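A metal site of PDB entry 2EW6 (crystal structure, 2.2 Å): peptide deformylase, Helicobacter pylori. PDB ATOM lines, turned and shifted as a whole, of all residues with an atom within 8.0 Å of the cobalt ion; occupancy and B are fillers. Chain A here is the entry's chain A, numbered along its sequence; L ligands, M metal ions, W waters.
Gln 50 touches the cobalt ion.
OE2 of Glu 138 touches the cobalt ion, at 3.9 Å.
The nearest printed residue that does not touch the cobalt ion is Leu 96 (4.7 Å).
N of Gly 45 sits close to O4 of the ligand (3.3 Å).
The cobalt ion is bound by NE2 of His 137, water W1, NE2 of His 141 and SG of Cys 95.
ND1 of His 137 sits at hydrogen-bond distance from OE1 of Glu 93 (2.8 Å).
The side-chain sulfur (SG) of Cys 95 sits close to the side-chain amide nitrogen (NE2) of Gln 50, at 3.6 Å.
N of Ser 97 sits close to SG of Cys 95 (3.5 Å).
The side-chain amide oxygen (OE1) of Gln 50 lies close to the side-chain carboxylate (OE1) of Glu 138 (3.5 Å).
The side-chain amide nitrogen (NE2) of Gln 50 lies within hydrogen-bond range of the side-chain hydroxyl (OG) of Ser 97 (3.0 Å).
OE1 of Gln 50 sits at hydrogen-bond distance from N of Ala 47 (2.8 Å).
The side-chain carboxylate (OE1) of Glu 138 lies within hydrogen-bond range of the backbone NH (N) of Ala 47, at 3.2 Å.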
ATOM      1  N   LEU A  13     -20.878  -1.586  19.324  1.00  0.00           N
ATOM      2  CA  LEU A  13     -20.420  -2.846  18.753  1.00  0.00           C
ATOM      3  C   LEU A  13     -21.573  -3.729  18.260  1.00  0.00           C
ATOM      4  O   LEU A  13     -21.344  -4.774  17.649  1.00  0.00           O
ATOM      5  CB  LEU A  13     -19.565  -3.601  19.779  1.00  0.00           C
ATOM      6  CG  LEU A  13     -18.261  -2.876  20.177  1.00  0.00           C
ATOM      7  CD1 LEU A  13     -17.519  -3.670  21.252  1.00  0.00           C
ATOM      8  CD2 LEU A  13     -17.392  -2.692  18.951  1.00  0.00           C
ATOM      9  N   GLY A  45      -6.419  -8.579  13.460  1.00  0.00           N
ATOM     10  CA  GLY A  45      -7.641  -8.267  12.738  1.00  0.00           C
ATOM     11  C   GLY A  45      -8.374  -7.072  13.338  1.00  0.00           C
ATOM     12  O   GLY A  45      -8.319  -6.846  14.548  1.00  0.00           O
ATOM     13  N   LEU A  46      -9.058  -6.294  12.487  1.00  0.00           N
ATOM     14  CA  LEU A  46      -9.801  -5.137  12.968  1.00  0.00           C
ATOM     15  C   LEU A  46     -10.925  -4.730  12.007  1.00  0.00           C
ATOM     16  O   LEU A  46     -10.705  -4.607  10.801  1.00  0.00           O
ATOM     17  CB  LEU A  46      -8.866  -3.939  13.176  1.00  0.00           C
ATOM     18  CG  LEU A  46      -9.529  -2.672  13.722  1.00  0.00           C
ATOM     19  CD1 LEU A  46      -9.956  -2.912  15.172  1.00  0.00           C
ATOM     20  CD2 LEU A  46      -8.572  -1.487  13.635  1.00  0.00           C
ATOM     21  N   ALA A  47     -12.118  -4.542  12.546  1.00  0.00           N
ATOM     22  CA  ALA A  47     -13.281  -4.138  11.761  1.00  0.00           C
ATOM     23  C   ALA A  47     -13.543  -2.661  12.004  1.00  0.00           C
ATOM     24  O   ALA A  47     -13.149  -2.107  13.034  1.00  0.00           O
ATOM     25  CB  ALA A  47     -14.493  -4.957  12.178  1.00  0.00           C
ATOM     26  N   ILE A  49     -16.300  -0.816  12.848  1.00  0.00           N
ATOM     27  CA  ILE A  49     -17.016  -0.358  14.043  1.00  0.00           C
ATOM     28  C   ILE A  49     -16.158  -0.380  15.288  1.00  0.00           C
ATOM     29  O   ILE A  49     -16.445   0.329  16.250  1.00  0.00           O
ATOM     30  CB  ILE A  49     -18.291  -1.196  14.385  1.00  0.00           C
ATOM     31  CG1 ILE A  49     -18.256  -2.514  13.632  1.00  0.00           C
ATOM     32  CG2 ILE A  49     -19.536  -0.352  14.164  1.00  0.00           C
ATOM     33  CD1 ILE A  49     -17.279  -3.507  14.209  1.00  0.00           C
ATOM     34  N   GLN A  50     -15.100  -1.189  15.279  1.00  0.00           N
ATOM     35  CA  GLN A  50     -14.205  -1.256  16.425  1.00  0.00           C
ATOM     36  C   GLN A  50     -13.515   0.085  16.660  1.00  0.00           C
ATOM     37  O   GLN A  50     -12.886   0.288  17.701  1.00  0.00           O
ATOM     38  CB  GLN A  50     -13.185  -2.374  16.229  1.00  0.00           C
ATOM     39  CG  GLN A  50     -13.757  -3.759  16.470  1.00  0.00           C
ATOM     40  CD  GLN A  50     -12.728  -4.851  16.359  1.00  0.00           C
ATOM     41  OE1 GLN A  50     -12.345  -5.253  15.261  1.00  0.00           O
ATOM     42  NE2 GLN A  50     -12.254  -5.329  17.504  1.00  0.00           N
ATOM     43  N   GLU A  93     -10.338 -17.771  20.518  1.00  0.00           N
ATOM     44  CA  GLU A  93     -10.236 -16.434  19.952  1.00  0.00           C
ATOM     45  C   GLU A  93     -10.062 -15.312  20.962  1.00  0.00           C
ATOM     46  O   GLU A  93     -10.309 -15.468  22.157  1.00  0.00           O
ATOM     47  CB  GLU A  93     -11.474 -16.171  19.106  1.00  0.00           C
ATOM     48  CG  GLU A  93     -11.599 -17.094  17.909  1.00  0.00           C
ATOM     49  CD  GLU A  93     -12.812 -16.772  17.056  1.00  0.00           C
ATOM     50  OE1 GLU A  93     -13.265 -15.614  17.083  1.00  0.00           O
ATOM     51  OE2 GLU A  93     -13.295 -17.687  16.357  1.00  0.00           O
ATOM     52  N   GLY A  94      -9.602 -14.175  20.444  1.00  0.00           N
ATOM     53  CA  GLY A  94      -9.388 -12.975  21.247  1.00  0.00           C
ATOM     54  C   GLY A  94      -9.963 -11.825  20.432  1.00  0.00           C
ATOM     55  O   GLY A  94     -10.390 -12.042  19.296  1.00  0.00           O
ATOM     56  N   CYS A  95      -9.959 -10.609  20.976  1.00  0.00           N
ATOM     57  CA  CYS A  95     -10.522  -9.468  20.266  1.00  0.00           C
ATOM     58  C   CYS A  95     -10.053  -8.160  20.906  1.00  0.00           C
ATOM     59  O   CYS A  95     -10.052  -8.031  22.129  1.00  0.00           O
ATOM     60  CB  CYS A  95     -12.066  -9.541  20.335  1.00  0.00           C
ATOM     61  SG  CYS A  95     -12.975  -8.301  19.362  1.00  0.00           S
ATOM     62  N   LEU A  96      -9.641  -7.192  20.083  1.00  0.00           N
ATOM     63  CA  LEU A  96      -9.195  -5.902  20.594  1.00  0.00           C
ATOM     64  C   LEU A  96     -10.331  -5.190  21.336  1.00  0.00           C
ATOM     65  O   LEU A  96     -10.089  -4.328  22.174  1.00  0.00           O
ATOM     66  CB  LEU A  96      -8.669  -5.012  19.457  1.00  0.00           C
ATOM     67  CG  LEU A  96      -7.307  -5.397  18.870  1.00  0.00           C
ATOM     68  CD1 LEU A  96      -6.962  -4.461  17.731  1.00  0.00           C
ATOM     69  CD2 LEU A  96      -6.244  -5.318  19.950  1.00  0.00           C
ATOM     70  N   SER A  97     -11.569  -5.551  21.005  1.00  0.00           N
ATOM     71  CA  SER A  97     -12.705  -4.922  21.683  1.00  0.00           C
ATOM     72  C   SER A  97     -13.081  -5.663  22.963  1.00  0.00           C
ATOM     73  O   SER A  97     -13.944  -5.200  23.712  1.00  0.00           O
ATOM     74  CB  SER A  97     -13.909  -4.837  20.752  1.00  0.00           C
ATOM     75  OG  SER A  97     -13.663  -3.900  19.728  1.00  0.00           O
ATOM     76  N   VAL A  98     -12.425  -6.787  23.222  1.00  0.00           N
ATOM     77  CA  VAL A  98     -12.679  -7.586  24.412  1.00  0.00           C
ATOM     78  C   VAL A  98     -11.316  -8.030  24.951  1.00  0.00           C
ATOM     79  O   VAL A  98     -11.035  -9.223  25.073  1.00  0.00           O
ATOM     80  CB  VAL A  98     -13.530  -8.838  24.088  1.00  0.00           C
ATOM     81  CG1 VAL A  98     -14.066  -9.470  25.372  1.00  0.00           C
ATOM     82  CG2 VAL A  98     -14.683  -8.471  23.157  1.00  0.00           C
ATOM     83  N   ARG A 107     -16.196 -22.478  14.504  1.00  0.00           N
ATOM     84  CA  ARG A 107     -16.130 -21.801  13.215  1.00  0.00           C
ATOM     85  C   ARG A 107     -16.113 -22.793  12.066  1.00  0.00           C
ATOM     86  O   ARG A 107     -15.783 -23.966  12.261  1.00  0.00           O
ATOM     87  CB  ARG A 107     -14.856 -20.965  13.133  1.00  0.00           C
ATOM     88  CG  ARG A 107     -14.726 -19.869  14.181  1.00  0.00           C
ATOM     89  CD  ARG A 107     -15.725 -18.749  13.930  1.00  0.00           C
ATOM     90  NE  ARG A 107     -15.502 -17.626  14.821  1.00  0.00           N
ATOM     91  CZ  ARG A 107     -16.249 -16.523  14.838  1.00  0.00           C
ATOM     92  NH1 ARG A 107     -17.270 -16.401  13.996  1.00  0.00           N
ATOM     93  NH2 ARG A 107     -15.982 -15.552  15.692  1.00  0.00           N
ATOM     94  N   ALA A 134     -10.254 -15.613  11.225  1.00  0.00           N
ATOM     95  CA  ALA A 134     -10.199 -14.155  11.286  1.00  0.00           C
ATOM     96  C   ALA A 134     -11.268 -13.537  10.404  1.00  0.00           C
ATOM     97  O   ALA A 134     -11.916 -12.557  10.782  1.00  0.00           O
ATOM     98  CB  ALA A 134      -8.811 -13.671  10.853  1.00  0.00           C
ATOM     99  N   HIS A 137     -14.623 -14.034  12.110  1.00  0.00           N
ATOM    100  CA  HIS A 137     -14.656 -13.188  13.297  1.00  0.00           C
ATOM    101  C   HIS A 137     -14.889 -11.730  12.898  1.00  0.00           C
ATOM    102  O   HIS A 137     -15.798 -11.078  13.405  1.00  0.00           O
ATOM    103  CB  HIS A 137     -13.315 -13.323  14.039  1.00  0.00           C
ATOM    104  CG  HIS A 137     -13.189 -12.433  15.232  1.00  0.00           C
ATOM    105  ND1 HIS A 137     -13.386 -12.888  16.524  1.00  0.00           N
ATOM    106  CD2 HIS A 137     -12.807 -11.138  15.353  1.00  0.00           C
ATOM    107  CE1 HIS A 137     -13.133 -11.918  17.374  1.00  0.00           C
ATOM    108  NE2 HIS A 137     -12.789 -10.846  16.693  1.00  0.00           N
ATOM    109  N   GLU A 138     -14.072 -11.222  11.978  1.00  0.00           N
ATOM    110  CA  GLU A 138     -14.211  -9.834  11.547  1.00  0.00           C
ATOM    111  C   GLU A 138     -15.562  -9.557  10.884  1.00  0.00           C
ATOM    112  O   GLU A 138     -16.175  -8.534  11.141  1.00  0.00           O
ATOM    113  CB  GLU A 138     -13.063  -9.455  10.600  1.00  0.00           C
ATOM    114  CG  GLU A 138     -11.697  -9.407  11.263  1.00  0.00           C
ATOM    115  CD  GLU A 138     -11.707  -8.701  12.609  1.00  0.00           C
ATOM    116  OE1 GLU A 138     -12.403  -7.677  12.748  1.00  0.00           O
ATOM    117  OE2 GLU A 138     -11.017  -9.172  13.532  1.00  0.00           O
ATOM    118  N   ILE A 139     -16.012 -10.469  10.039  1.00  0.00           N
ATOM    119  CA  ILE A 139     -17.300 -10.288   9.384  1.00  0.00           C
ATOM    120  C   ILE A 139     -18.425 -10.249  10.424  1.00  0.00           C
ATOM    121  O   ILE A 139     -19.419  -9.548  10.247  1.00  0.00           O
ATOM    122  CB  ILE A 139     -17.554 -11.383   8.309  1.00  0.00           C
ATOM    123  CG1 ILE A 139     -16.749 -11.048   7.048  1.00  0.00           C
ATOM    124  CG2 ILE A 139     -19.036 -11.466   7.968  1.00  0.00           C
ATOM    125  CD1 ILE A 139     -16.863 -12.071   5.934  1.00  0.00           C
ATOM    126  N   ASP A 140     -18.273 -11.005  11.515  1.00  0.00           N
ATOM    127  CA  ASP A 140     -19.290 -10.983  12.562  1.00  0.00           C
ATOM    128  C   ASP A 140     -19.422  -9.547  13.100  1.00  0.00           C
ATOM    129  O   ASP A 140     -20.516  -9.097  13.428  1.00  0.00           O
ATOM    130  CB  ASP A 140     -18.935 -11.924  13.714  1.00  0.00           C
ATOM    131  CG  ASP A 140     -19.430 -13.351  13.483  1.00  0.00           C
ATOM    132  OD1 ASP A 140     -20.364 -13.553  12.671  1.00  0.00           O
ATOM    133  OD2 ASP A 140     -18.896 -14.269  14.126  1.00  0.00           O
ATOM    134  N   HIS A 141     -18.300  -8.837  13.179  1.00  0.00           N
ATOM    135  CA  HIS A 141     -18.334  -7.456  13.667  1.00  0.00           C
ATOM    136  C   HIS A 141     -19.217  -6.584  12.801  1.00  0.00           C
ATOM    137  O   HIS A 141     -19.938  -5.724  13.311  1.00  0.00           O
ATOM    138  CB  HIS A 141     -16.917  -6.859  13.690  1.00  0.00           C
ATOM    139  CG  HIS A 141     -16.144  -7.183  14.926  1.00  0.00           C
ATOM    140  ND1 HIS A 141     -16.587  -6.882  16.190  1.00  0.00           N
ATOM    141  CD2 HIS A 141     -14.936  -7.769  15.089  1.00  0.00           C
ATOM    142  CE1 HIS A 141     -15.691  -7.254  17.073  1.00  0.00           C
ATOM    143  NE2 HIS A 141     -14.679  -7.799  16.431  1.00  0.00           N
ATOM    144  N   VAL A 145     -21.863  -8.639  15.787  1.00  0.00           N
ATOM    145  CA  VAL A 145     -21.630  -9.867  16.544  1.00  0.00           C
ATOM    146  C   VAL A 145     -20.219  -9.973  17.132  1.00  0.00           C
ATOM    147  O   VAL A 145     -19.227  -9.778  16.426  1.00  0.00           O
ATOM    148  CB  VAL A 145     -21.892 -11.110  15.662  1.00  0.00           C
ATOM    149  CG1 VAL A 145     -21.542 -12.379  16.413  1.00  0.00           C
ATOM    150  CG2 VAL A 145     -23.348 -11.137  15.239  1.00  0.00           C
ATOM    151  N   LEU A 146     -20.148 -10.278  18.426  1.00  0.00           N
ATOM    152  CA  LEU A 146     -18.871 -10.432  19.129  1.00  0.00           C
ATOM    153  C   LEU A 146     -18.669 -11.927  19.374  1.00  0.00           C
ATOM    154  O   LEU A 146     -19.648 -12.666  19.466  1.00  0.00           O
ATOM    155  CB  LEU A 146     -18.906  -9.687  20.457  1.00  0.00           C
ATOM    156  CG  LEU A 146     -19.157  -8.172  20.362  1.00  0.00           C
ATOM    157  CD1 LEU A 146     -19.205  -7.565  21.748  1.00  0.00           C
ATOM    158  CD2 LEU A 146     -18.048  -7.532  19.531  1.00  0.00           C
ATOM    159  N   PHE A 147     -17.422 -12.381  19.463  1.00  0.00           N
ATOM    160  CA  PHE A 147     -17.197 -13.804  19.674  1.00  0.00           C
ATOM    161  C   PHE A 147     -17.744 -14.315  21.006  1.00  0.00           C
ATOM    162  O   PHE A 147     -18.046 -15.500  21.148  1.00  0.00           O
ATOM    163  CB  PHE A 147     -15.708 -14.163  19.525  1.00  0.00           C
ATOM    164  CG  PHE A 147     -14.866 -13.821  20.719  1.00  0.00           C
ATOM    165  CD1 PHE A 147     -14.434 -12.518  20.941  1.00  0.00           C
ATOM    166  CD2 PHE A 147     -14.467 -14.817  21.611  1.00  0.00           C
ATOM    167  CE1 PHE A 147     -13.614 -12.208  22.034  1.00  0.00           C
ATOM    168  CE2 PHE A 147     -13.661 -14.516  22.704  1.00  0.00           C
ATOM    169  CZ  PHE A 147     -13.225 -13.209  22.909  1.00  0.00           C
HETATM  170  C1  LIG L   1      -8.335 -15.546  15.881  1.00  0.00           C
HETATM  171  O1  LIG L   1      -7.987 -16.883  16.059  1.00  0.00           O
HETATM  172  C2  LIG L   1      -9.030 -14.812  16.889  1.00  0.00           C
HETATM  173  C3  LIG L   1      -9.379 -13.453  16.680  1.00  0.00           C
HETATM  174  C4  LIG L   1      -9.030 -12.799  15.454  1.00  0.00           C
HETATM  175  C5  LIG L   1      -9.399 -11.333  15.242  1.00  0.00           C
HETATM  176  C6  LIG L   1      -8.193 -10.426  15.594  1.00  0.00           C
HETATM  177  N1  LIG L   1      -8.071 -10.376  17.054  1.00  0.00           N
HETATM  178  C7  LIG L   1      -7.098  -9.662  17.504  1.00  0.00           C
HETATM  179  C8  LIG L   1      -6.930  -9.578  18.985  1.00  0.00           C
HETATM  180  C9  LIG L   1      -5.965  -8.863  19.600  1.00  0.00           C
HETATM  181  C10 LIG L   1      -5.753  -8.730  21.113  1.00  0.00           C
HETATM  182  C11 LIG L   1      -4.590  -8.011  21.558  1.00  0.00           C
HETATM  183  C12 LIG L   1      -4.335  -7.837  22.944  1.00  0.00           C
HETATM  184  C13 LIG L   1      -5.217  -8.372  23.927  1.00  0.00           C
HETATM  185  O2  LIG L   1      -4.968  -8.200  25.306  1.00  0.00           O
HETATM  186  C14 LIG L   1      -6.384  -9.096  23.499  1.00  0.00           C
HETATM  187  O3  LIG L   1      -7.252  -9.618  24.458  1.00  0.00           O
HETATM  188  C15 LIG L   1      -6.643  -9.262  22.101  1.00  0.00           C
HETATM  189  O4  LIG L   1      -6.309  -9.051  16.772  1.00  0.00           O
HETATM  190  C16 LIG L   1      -8.342 -13.530  14.450  1.00  0.00           C
HETATM  191  C17 LIG L   1      -7.994 -14.889  14.659  1.00  0.00           C
HETATM  192 CO    CO M   1     -12.800  -8.727  17.027  1.00  0.00          CO
HETATM  193  O   HOH W   1     -11.387  -7.813  15.646  1.00  0.00           O
